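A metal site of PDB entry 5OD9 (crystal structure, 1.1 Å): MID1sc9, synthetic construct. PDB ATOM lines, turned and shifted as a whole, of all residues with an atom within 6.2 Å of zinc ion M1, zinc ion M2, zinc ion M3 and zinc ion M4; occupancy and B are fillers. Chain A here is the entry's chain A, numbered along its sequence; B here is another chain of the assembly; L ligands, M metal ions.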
ATOM      1  N   GLN A  33      17.637  -6.086  16.713  1.00  0.00           N
ATOM      2  CA  GLN A  33      17.466  -6.811  15.439  1.00  0.00           C
ATOM      3  C   GLN A  33      17.324  -5.846  14.258  1.00  0.00           C
ATOM      4  O   GLN A  33      17.892  -6.066  13.186  1.00  0.00           O
ATOM      5  CB  GLN A  33      16.291  -7.733  15.563  1.00  0.00           C
ATOM      6  CG  GLN A  33      16.546  -8.948  16.504  1.00  0.00           C
ATOM      7  CD  GLN A  33      15.341  -9.849  16.638  1.00  0.00           C
ATOM      8  OE1 GLN A  33      14.204  -9.355  16.552  1.00  0.00           O
ATOM      9  NE2 GLN A  33      15.530 -11.111  16.942  1.00  0.00           N
ATOM     10  N   GLU A  34      16.545  -4.792  14.463  1.00  0.00           N
ATOM     11  CA  GLU A  34      16.291  -3.880  13.357  1.00  0.00           C
ATOM     12  C   GLU A  34      17.545  -3.106  12.992  1.00  0.00           C
ATOM     13  O   GLU A  34      17.749  -2.807  11.805  1.00  0.00           O
ATOM     14  CB  GLU A  34      15.106  -2.973  13.757  1.00  0.00           C
ATOM     15  CG  GLU A  34      13.821  -3.804  13.798  1.00  0.00           C
ATOM     16  CD  GLU A  34      12.596  -3.053  14.254  1.00  0.00           C
ATOM     17  OE1 GLU A  34      12.722  -1.980  14.819  1.00  0.00           O
ATOM     18  OE2 GLU A  34      11.529  -3.650  14.042  1.00  0.00           O
ATOM     19  N   HIS A  37      19.417  -5.655  10.863  1.00  0.00           N
ATOM     20  CA  HIS A  37      18.763  -6.049   9.585  1.00  0.00           C
ATOM     21  C   HIS A  37      19.530  -5.677   8.326  1.00  0.00           C
ATOM     22  O   HIS A  37      19.842  -6.601   7.538  1.00  0.00           O
ATOM     23  CB  HIS A  37      17.320  -5.525   9.622  1.00  0.00           C
ATOM     24  CG  HIS A  37      16.466  -5.855   8.462  1.00  0.00           C
ATOM     25  ND1 HIS A  37      15.431  -6.784   8.540  1.00  0.00           N
ATOM     26  CD2 HIS A  37      16.476  -5.406   7.169  1.00  0.00           C
ATOM     27  CE1 HIS A  37      14.887  -6.820   7.338  1.00  0.00           C
ATOM     28  NE2 HIS A  37      15.481  -6.018   6.443  1.00  0.00           N
ATOM     29  N   TRP A  40      23.130  -7.640   8.371  1.00  0.00           N
ATOM     30  CA  TRP A  40      23.001  -9.060   8.078  1.00  0.00           C
ATOM     31  C   TRP A  40      22.608  -9.307   6.636  1.00  0.00           C
ATOM     32  O   TRP A  40      23.159 -10.197   5.983  1.00  0.00           O
ATOM     33  CB  TRP A  40      21.961  -9.687   9.027  1.00  0.00           C
ATOM     34  CG  TRP A  40      21.574 -11.054   8.591  1.00  0.00           C
ATOM     35  CD1 TRP A  40      20.327 -11.419   8.128  1.00  0.00           C
ATOM     36  CD2 TRP A  40      22.355 -12.244   8.544  1.00  0.00           C
ATOM     37  NE1 TRP A  40      20.301 -12.733   7.796  1.00  0.00           N
ATOM     38  CE2 TRP A  40      21.539 -13.272   8.043  1.00  0.00           C
ATOM     39  CE3 TRP A  40      23.710 -12.560   8.877  1.00  0.00           C
ATOM     40  CZ2 TRP A  40      21.995 -14.558   7.865  1.00  0.00           C
ATOM     41  CZ3 TRP A  40      24.152 -13.841   8.700  1.00  0.00           C
ATOM     42  CH2 TRP A  40      23.297 -14.798   8.200  1.00  0.00           C
ATOM     43  N   HIS A  41      21.707  -8.520   6.078  1.00  0.00           N
ATOM     44  CA  HIS A  41      21.371  -8.763   4.675  1.00  0.00           C
ATOM     45  C   HIS A  41      22.507  -8.461   3.724  1.00  0.00           C
ATOM     46  O   HIS A  41      22.731  -9.215   2.787  1.00  0.00           O
ATOM     47  CB  HIS A  41      20.125  -7.955   4.330  1.00  0.00           C
ATOM     48  CG  HIS A  41      18.891  -8.686   4.787  1.00  0.00           C
ATOM     49  ND1 HIS A  41      17.647  -8.087   4.799  1.00  0.00           N
ATOM     50  CD2 HIS A  41      18.709  -9.966   5.205  1.00  0.00           C
ATOM     51  CE1 HIS A  41      16.779  -8.988   5.235  1.00  0.00           C
ATOM     52  NE2 HIS A  41      17.341 -10.137   5.503  1.00  0.00           N
ATOM     53  N   GLU A  60      18.677 -17.279   7.951  1.00  0.00           N
ATOM     54  CA  GLU A  60      17.912 -16.278   7.206  1.00  0.00           C
ATOM     55  C   GLU A  60      16.430 -16.610   7.155  1.00  0.00           C
ATOM     56  O   GLU A  60      15.576 -15.718   7.270  1.00  0.00           O
ATOM     57  CB  GLU A  60      18.547 -16.072   5.818  1.00  0.00           C
ATOM     58  CG  GLU A  60      17.742 -15.194   4.912  1.00  0.00           C
ATOM     59  CD  GLU A  60      17.326 -13.817   5.453  1.00  0.00           C
ATOM     60  OE1 GLU A  60      17.983 -13.298   6.342  1.00  0.00           O
ATOM     61  OE2 GLU A  60      16.305 -13.294   5.011  1.00  0.00           O
ATOM     62  N   HIS A  63      14.984 -15.367  10.297  1.00  0.00           N
ATOM     63  CA  HIS A  63      14.772 -13.953  10.200  1.00  0.00           C
ATOM     64  C   HIS A  63      13.472 -13.608   9.466  1.00  0.00           C
ATOM     65  O   HIS A  63      12.722 -12.783   9.946  1.00  0.00           O
ATOM     66  CB  HIS A  63      16.003 -13.342   9.475  1.00  0.00           C
ATOM     67  CG  HIS A  63      15.931 -11.830   9.433  1.00  0.00           C
ATOM     68  ND1 HIS A  63      16.411 -11.159   8.279  1.00  0.00           N
ATOM     69  CD2 HIS A  63      15.531 -10.907  10.317  1.00  0.00           C
ATOM     70  CE1 HIS A  63      16.253  -9.863   8.581  1.00  0.00           C
ATOM     71  NE2 HIS A  63      15.735  -9.640   9.783  1.00  0.00           N
ATOM     72  N   VAL A  64      13.245 -14.257   8.344  1.00  0.00           N
ATOM     73  CA  VAL A  64      11.970 -14.058   7.639  1.00  0.00           C
ATOM     74  C   VAL A  64      10.822 -14.385   8.571  1.00  0.00           C
ATOM     75  O   VAL A  64       9.820 -13.607   8.616  1.00  0.00           O
ATOM     76  CB  VAL A  64      11.946 -14.968   6.393  1.00  0.00           C
ATOM     77  CG1 VAL A  64      10.560 -15.047   5.802  1.00  0.00           C
ATOM     78  CG2 VAL A  64      12.967 -14.494   5.349  1.00  0.00           C
ATOM     79  N   HIS A  67      10.117 -11.743  11.222  1.00  0.00           N
ATOM     80  CA  HIS A  67       9.324 -10.660  10.724  1.00  0.00           C
ATOM     81  C   HIS A  67       7.857 -11.032  10.682  1.00  0.00           C
ATOM     82  O   HIS A  67       6.983 -10.260  11.058  1.00  0.00           O
ATOM     83  CB  HIS A  67       9.763 -10.238   9.312  1.00  0.00           C
ATOM     84  CG  HIS A  67      10.894  -9.299   9.267  1.00  0.00           C
ATOM     85  ND1 HIS A  67      10.869  -8.080   8.598  1.00  0.00           N
ATOM     86  CD2 HIS A  67      12.091  -9.364   9.881  1.00  0.00           C
ATOM     87  CE1 HIS A  67      12.040  -7.493   8.811  1.00  0.00           C
ATOM     88  NE2 HIS A  67      12.831  -8.225   9.589  1.00  0.00           N
ATOM     89  N   GLN A  68       7.550 -12.240  10.271  1.00  0.00           N
ATOM     90  CA  GLN A  68       6.150 -12.651  10.161  1.00  0.00           C
ATOM     91  C   GLN A  68       5.493 -12.780  11.537  1.00  0.00           C
ATOM     92  O   GLN A  68       4.372 -12.355  11.706  1.00  0.00           O
ATOM     93  CB  GLN A  68       5.988 -13.946   9.363  1.00  0.00           C
ATOM     94  CG  GLN A  68       6.410 -13.695   7.904  1.00  0.00           C
ATOM     95  CD  GLN A  68       5.418 -13.103   6.943  1.00  0.00           C
ATOM     96  OE1 GLN A  68       4.245 -13.480   6.859  1.00  0.00           O
ATOM     97  NE2 GLN A  68       5.812 -12.139   6.100  1.00  0.00           N
ATOM     98  N   ARG A  70       6.429 -11.213  14.285  1.00  0.00           N
ATOM     99  CA  ARG A  70       6.314  -9.871  14.881  1.00  0.00           C
ATOM    100  C   ARG A  70       5.099  -9.194  14.247  1.00  0.00           C
ATOM    101  O   ARG A  70       4.353  -8.546  15.010  1.00  0.00           O
ATOM    102  CB  ARG A  70       7.637  -9.091  14.720  1.00  0.00           C
ATOM    103  CG  ARG A  70       7.669  -7.603  14.906  1.00  0.00           C
ATOM    104  CD  ARG A  70       9.151  -7.147  15.067  1.00  0.00           C
ATOM    105  NE  ARG A  70       9.833  -7.688  16.240  1.00  0.00           N
ATOM    106  CZ  ARG A  70      11.022  -8.241  16.291  1.00  0.00           C
ATOM    107  NH1 ARG A  70      11.748  -8.333  15.171  1.00  0.00           N
ATOM    108  NH2 ARG A  70      11.517  -8.717  17.467  1.00  0.00           N
ATOM    109  N   GLN B  33      17.041   2.199   2.267  1.00  0.00           N
ATOM    110  CA  GLN B  33      15.886   1.435   1.885  1.00  0.00           C
ATOM    111  C   GLN B  33      15.634   0.305   2.859  1.00  0.00           C
ATOM    112  O   GLN B  33      14.513  -0.052   3.209  1.00  0.00           O
ATOM    113  CB  GLN B  33      16.135   0.829   0.491  1.00  0.00           C
ATOM    114  CG  GLN B  33      15.991   1.860  -0.623  1.00  0.00           C
ATOM    115  CD  GLN B  33      16.330   1.324  -2.005  1.00  0.00           C
ATOM    116  OE1 GLN B  33      16.812   0.175  -2.147  1.00  0.00           O
ATOM    117  NE2 GLN B  33      16.044   2.204  -2.967  1.00  0.00           N
ATOM    118  N   GLU B  34      16.727  -0.306   3.320  1.00  0.00           N
ATOM    119  CA  GLU B  34      16.654  -1.393   4.312  1.00  0.00           C
ATOM    120  C   GLU B  34      16.324  -0.871   5.692  1.00  0.00           C
ATOM    121  O   GLU B  34      15.566  -1.521   6.397  1.00  0.00           O
ATOM    122  CB  GLU B  34      17.907  -2.251   4.257  1.00  0.00           C
ATOM    123  CG  GLU B  34      17.762  -3.299   3.166  1.00  0.00           C
ATOM    124  CD  GLU B  34      16.923  -4.465   3.609  1.00  0.00           C
ATOM    125  OE1 GLU B  34      15.670  -4.267   3.691  1.00  0.00           O
ATOM    126  OE2 GLU B  34      17.540  -5.502   3.929  1.00  0.00           O
ATOM    127  N   HIS B  37      12.518  -0.648   5.927  1.00  0.00           N
ATOM    128  CA  HIS B  37      11.714  -1.859   6.078  1.00  0.00           C
ATOM    129  C   HIS B  37      11.244  -2.019   7.499  1.00  0.00           C
ATOM    130  O   HIS B  37      10.006  -2.069   7.667  1.00  0.00           O
ATOM    131  CB  HIS B  37      12.567  -2.962   5.425  1.00  0.00           C
ATOM    132  CG  HIS B  37      12.045  -4.344   5.575  1.00  0.00           C
ATOM    133  ND1 HIS B  37      12.773  -5.392   5.112  1.00  0.00           N
ATOM    134  CD2 HIS B  37      10.920  -4.869   6.101  1.00  0.00           C
ATOM    135  CE1 HIS B  37      12.050  -6.489   5.368  1.00  0.00           C
ATOM    136  NE2 HIS B  37      10.917  -6.217   5.993  1.00  0.00           N
ATOM    137  N   PRO B  38      12.081  -2.226   8.503  1.00  0.00           N
ATOM    138  CA  PRO B  38      11.492  -2.356   9.845  1.00  0.00           C
ATOM    139  C   PRO B  38      10.707  -1.126  10.269  1.00  0.00           C
ATOM    140  O   PRO B  38       9.761  -1.247  11.022  1.00  0.00           O
ATOM    141  CB  PRO B  38      12.666  -2.594  10.784  1.00  0.00           C
ATOM    142  CG  PRO B  38      13.858  -2.778   9.930  1.00  0.00           C
ATOM    143  CD  PRO B  38      13.512  -2.428   8.533  1.00  0.00           C
ATOM    144  N   HIS B  41       7.237  -1.474   9.003  1.00  0.00           N
ATOM    145  CA  HIS B  41       6.449  -2.426   9.764  1.00  0.00           C
ATOM    146  C   HIS B  41       5.992  -1.856  11.096  1.00  0.00           C
ATOM    147  O   HIS B  41       4.864  -2.120  11.502  1.00  0.00           O
ATOM    148  CB  HIS B  41       7.251  -3.698  10.049  1.00  0.00           C
ATOM    149  CG  HIS B  41       7.475  -4.647   8.949  1.00  0.00           C
ATOM    150  ND1 HIS B  41       6.593  -4.944   7.935  1.00  0.00           N
ATOM    151  CD2 HIS B  41       8.545  -5.453   8.695  1.00  0.00           C
ATOM    152  CE1 HIS B  41       7.078  -5.855   7.169  1.00  0.00           C
ATOM    153  NE2 HIS B  41       8.288  -6.214   7.598  1.00  0.00           N
ATOM    154  N   HIS B  63       7.225  -5.238   1.366  1.00  0.00           N
ATOM    155  CA  HIS B  63       8.343  -5.607   2.241  1.00  0.00           C
ATOM    156  C   HIS B  63       8.431  -7.094   2.503  1.00  0.00           C
ATOM    157  O   HIS B  63       9.529  -7.640   2.466  1.00  0.00           O
ATOM    158  CB  HIS B  63       8.275  -4.832   3.544  1.00  0.00           C
ATOM    159  CG  HIS B  63       8.572  -3.380   3.333  1.00  0.00           C
ATOM    160  ND1 HIS B  63       9.799  -2.867   3.101  1.00  0.00           N
ATOM    161  CD2 HIS B  63       7.694  -2.366   3.286  1.00  0.00           C
ATOM    162  CE1 HIS B  63       9.708  -1.545   2.931  1.00  0.00           C
ATOM    163  NE2 HIS B  63       8.422  -1.183   3.028  1.00  0.00           N
ATOM    164  N   VAL B  64       7.319  -7.754   2.738  1.00  0.00           N
ATOM    165  CA  VAL B  64       7.296  -9.225   2.905  1.00  0.00           C
ATOM    166  C   VAL B  64       7.958  -9.901   1.707  1.00  0.00           C
ATOM    167  O   VAL B  64       8.769 -10.804   1.845  1.00  0.00           O
ATOM    168  CB  VAL B  64       5.870  -9.761   3.177  1.00  0.00           C
ATOM    169  CG1 VAL B  64       5.835 -11.263   3.089  1.00  0.00           C
ATOM    170  CG2 VAL B  64       5.334  -9.253   4.491  1.00  0.00           C
ATOM    171  N   ILE B  66       9.933  -8.515  -0.699  1.00  0.00           N
ATOM    172  CA  ILE B  66      11.365  -8.162  -0.797  1.00  0.00           C
ATOM    173  C   ILE B  66      12.160  -9.118   0.077  1.00  0.00           C
ATOM    174  O   ILE B  66      13.189  -9.640  -0.351  1.00  0.00           O
ATOM    175  CB  ILE B  66      11.614  -6.736  -0.434  1.00  0.00           C
ATOM    176  CG1 ILE B  66      10.995  -5.734  -1.432  1.00  0.00           C
ATOM    177  CG2 ILE B  66      13.100  -6.459  -0.255  1.00  0.00           C
ATOM    178  CD1 ILE B  66      10.806  -4.362  -0.898  1.00  0.00           C
ATOM    179  N   HIS B  67      11.703  -9.330   1.312  1.00  0.00           N
ATOM    180  CA  HIS B  67      12.466 -10.159   2.225  1.00  0.00           C
ATOM    181  C   HIS B  67      12.571 -11.609   1.713  1.00  0.00           C
ATOM    182  O   HIS B  67      13.654 -12.214   1.745  1.00  0.00           O
ATOM    183  CB  HIS B  67      11.815 -10.108   3.619  1.00  0.00           C
ATOM    184  CG  HIS B  67      12.758 -10.547   4.708  1.00  0.00           C
ATOM    185  ND1 HIS B  67      12.446 -10.408   6.040  1.00  0.00           N
ATOM    186  CD2 HIS B  67      14.005 -11.028   4.699  1.00  0.00           C
ATOM    187  CE1 HIS B  67      13.467 -10.802   6.773  1.00  0.00           C
ATOM    188  NE2 HIS B  67      14.448 -11.171   5.986  1.00  0.00           N
ATOM    189  N   ARG B  70      15.014 -11.741  -1.096  1.00  0.00           N
ATOM    190  CA  ARG B  70      16.393 -11.668  -0.664  1.00  0.00           C
ATOM    191  C   ARG B  70      16.889 -12.981  -0.072  1.00  0.00           C
ATOM    192  O   ARG B  70      17.977 -13.426  -0.309  1.00  0.00           O
ATOM    193  CB  ARG B  70      16.542 -10.470   0.299  1.00  0.00           C
ATOM    194  CG  ARG B  70      17.992 -10.033   0.392  1.00  0.00           C
ATOM    195  CD  ARG B  70      18.170  -8.977   1.485  1.00  0.00           C
ATOM    196  NE  ARG B  70      17.207  -7.888   1.397  1.00  0.00           N
ATOM    197  CZ  ARG B  70      17.341  -6.764   0.705  1.00  0.00           C
ATOM    198  NH1 ARG B  70      18.401  -6.535   0.006  1.00  0.00           N
ATOM    199  NH2 ARG B  70      16.340  -5.891   0.770  1.00  0.00           N
ATOM    200  N   ALA B  71      16.003 -13.631   0.693  1.00  0.00           N
ATOM    201  CA  ALA B  71      16.370 -14.891   1.346  1.00  0.00           C
ATOM    202  C   ALA B  71      16.667 -15.963   0.287  1.00  0.00           C
ATOM    203  O   ALA B  71      17.467 -16.845   0.535  1.00  0.00           O
ATOM    204  CB  ALA B  71      15.248 -15.381   2.270  1.00  0.00           C
HETATM  205 CL1  LIG L   1      14.871  -7.068  12.119  1.00  0.00          CL
HETATM  206 CL1  LG2 L   2       9.213  -9.360   5.983  1.00  0.00          CL
HETATM  207 CL1  LG3 L   3      14.506  -7.481   3.272  1.00  0.00          CL
HETATM  208 ZN    ZN M   1      14.767  -7.896  10.068  1.00  0.00          ZN
HETATM  209 ZN    ZN M   2      16.409 -11.690   6.366  1.00  0.00          ZN
HETATM  210 ZN    ZN M   3       9.749  -7.482   7.026  1.00  0.00          ZN
HETATM  211 ZN    ZN M   4      14.706  -5.678   4.631  1.00  0.00          ZN
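A ring nitrogen (NE2) of His 37 of chain A sits close to a ring nitrogen (ND1) of His 41 of chain A, 3.4 Å away.
NE of Arg 70 of chain B is in hydrogen-bond range of ND1 of His 41 of chain A (3.4 Å).
The side-chain carboxylate of Glu 60 sits close to the indole nitrogen of Trp 40 (2.8 Å).
OE2 of Glu 34 of chain B lies within salt-bridge range of NH2 of Arg 70 of chain B (3.4 Å).
The side-chain carboxylate of Glu 34 of chain B sits at hydrogen-bond distance from a ring nitrogen (ND1) of His 41 of chain A, 2.7 Å away.
Three residues have an atom within 4 Å of zinc ion M1: His 37 of chain A, His 63 of chain A and His 67 of chain A.
Along chain A the residues within 4 Å of zinc ion M1 span positions 37 to 67.
The nearest printed residue that does not touch zinc ion M1 is His 67 of chain B (4.6 Å).
Within 4 Å of zinc ion M2: His 41 of chain A, Glu 60, His 63 of chain A and His 67 of chain B.
The nearest printed residue that does not touch zinc ion M2 is Trp 40 (4.3 Å).
Within 4 Å of zinc ion M3: His 67 of chain A, His 37 of chain B and His 41 of chain B.
Zinc ion M1 is bound by a ring nitrogen (ND1) of His 37 of chain A (2.0 Å), a ring nitrogen (NE2) of His 63 of chain A (2.0 Å), a ring nitrogen (NE2) of His 67 of chain A (2.0 Å) and a chlorine (CL1) of LIG L1 (2.2 Å).
Zinc ion M1 has four donor atoms within binding distance.
Zinc ion M2 is bound by ND1 of His 63 of chain A (2.0 Å), NE2 of His 41 of chain A (2.0 Å), NE2 of His 67 of chain B (2.1 Å), OE2 of Glu 60 (2.1 Å) and OE1 of Glu 60 (2.3 Å).
A ring nitrogen (NE2) of His 37 of chain B is bound to zinc ion M3 (2.0 Å).
NE2 of His 41 of chain B binds zinc ion M3 (2.0 Å).
Zinc ion M3 is bound by a ring nitrogen (ND1) of His 67 of chain A, at 2.0 Å.
Zinc ion M3 is bound by CL1 of LG2 L2, 2.2 Å away.
Zinc ion M3 has four donor atoms within binding distance.
Zinc ion M4 is bound by OE1 of Glu 34 of chain B.
NE2 of His 37 of chain A is bound to zinc ion M4 (2.0 Å).
ND1 of His 37 of chain B binds zinc ion M4, at 2.0 Å.
CL1 of LG3 L3 binds zinc ion M4, 2.3 Å away.
Zinc ion M4 has four donor atoms within binding distance.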
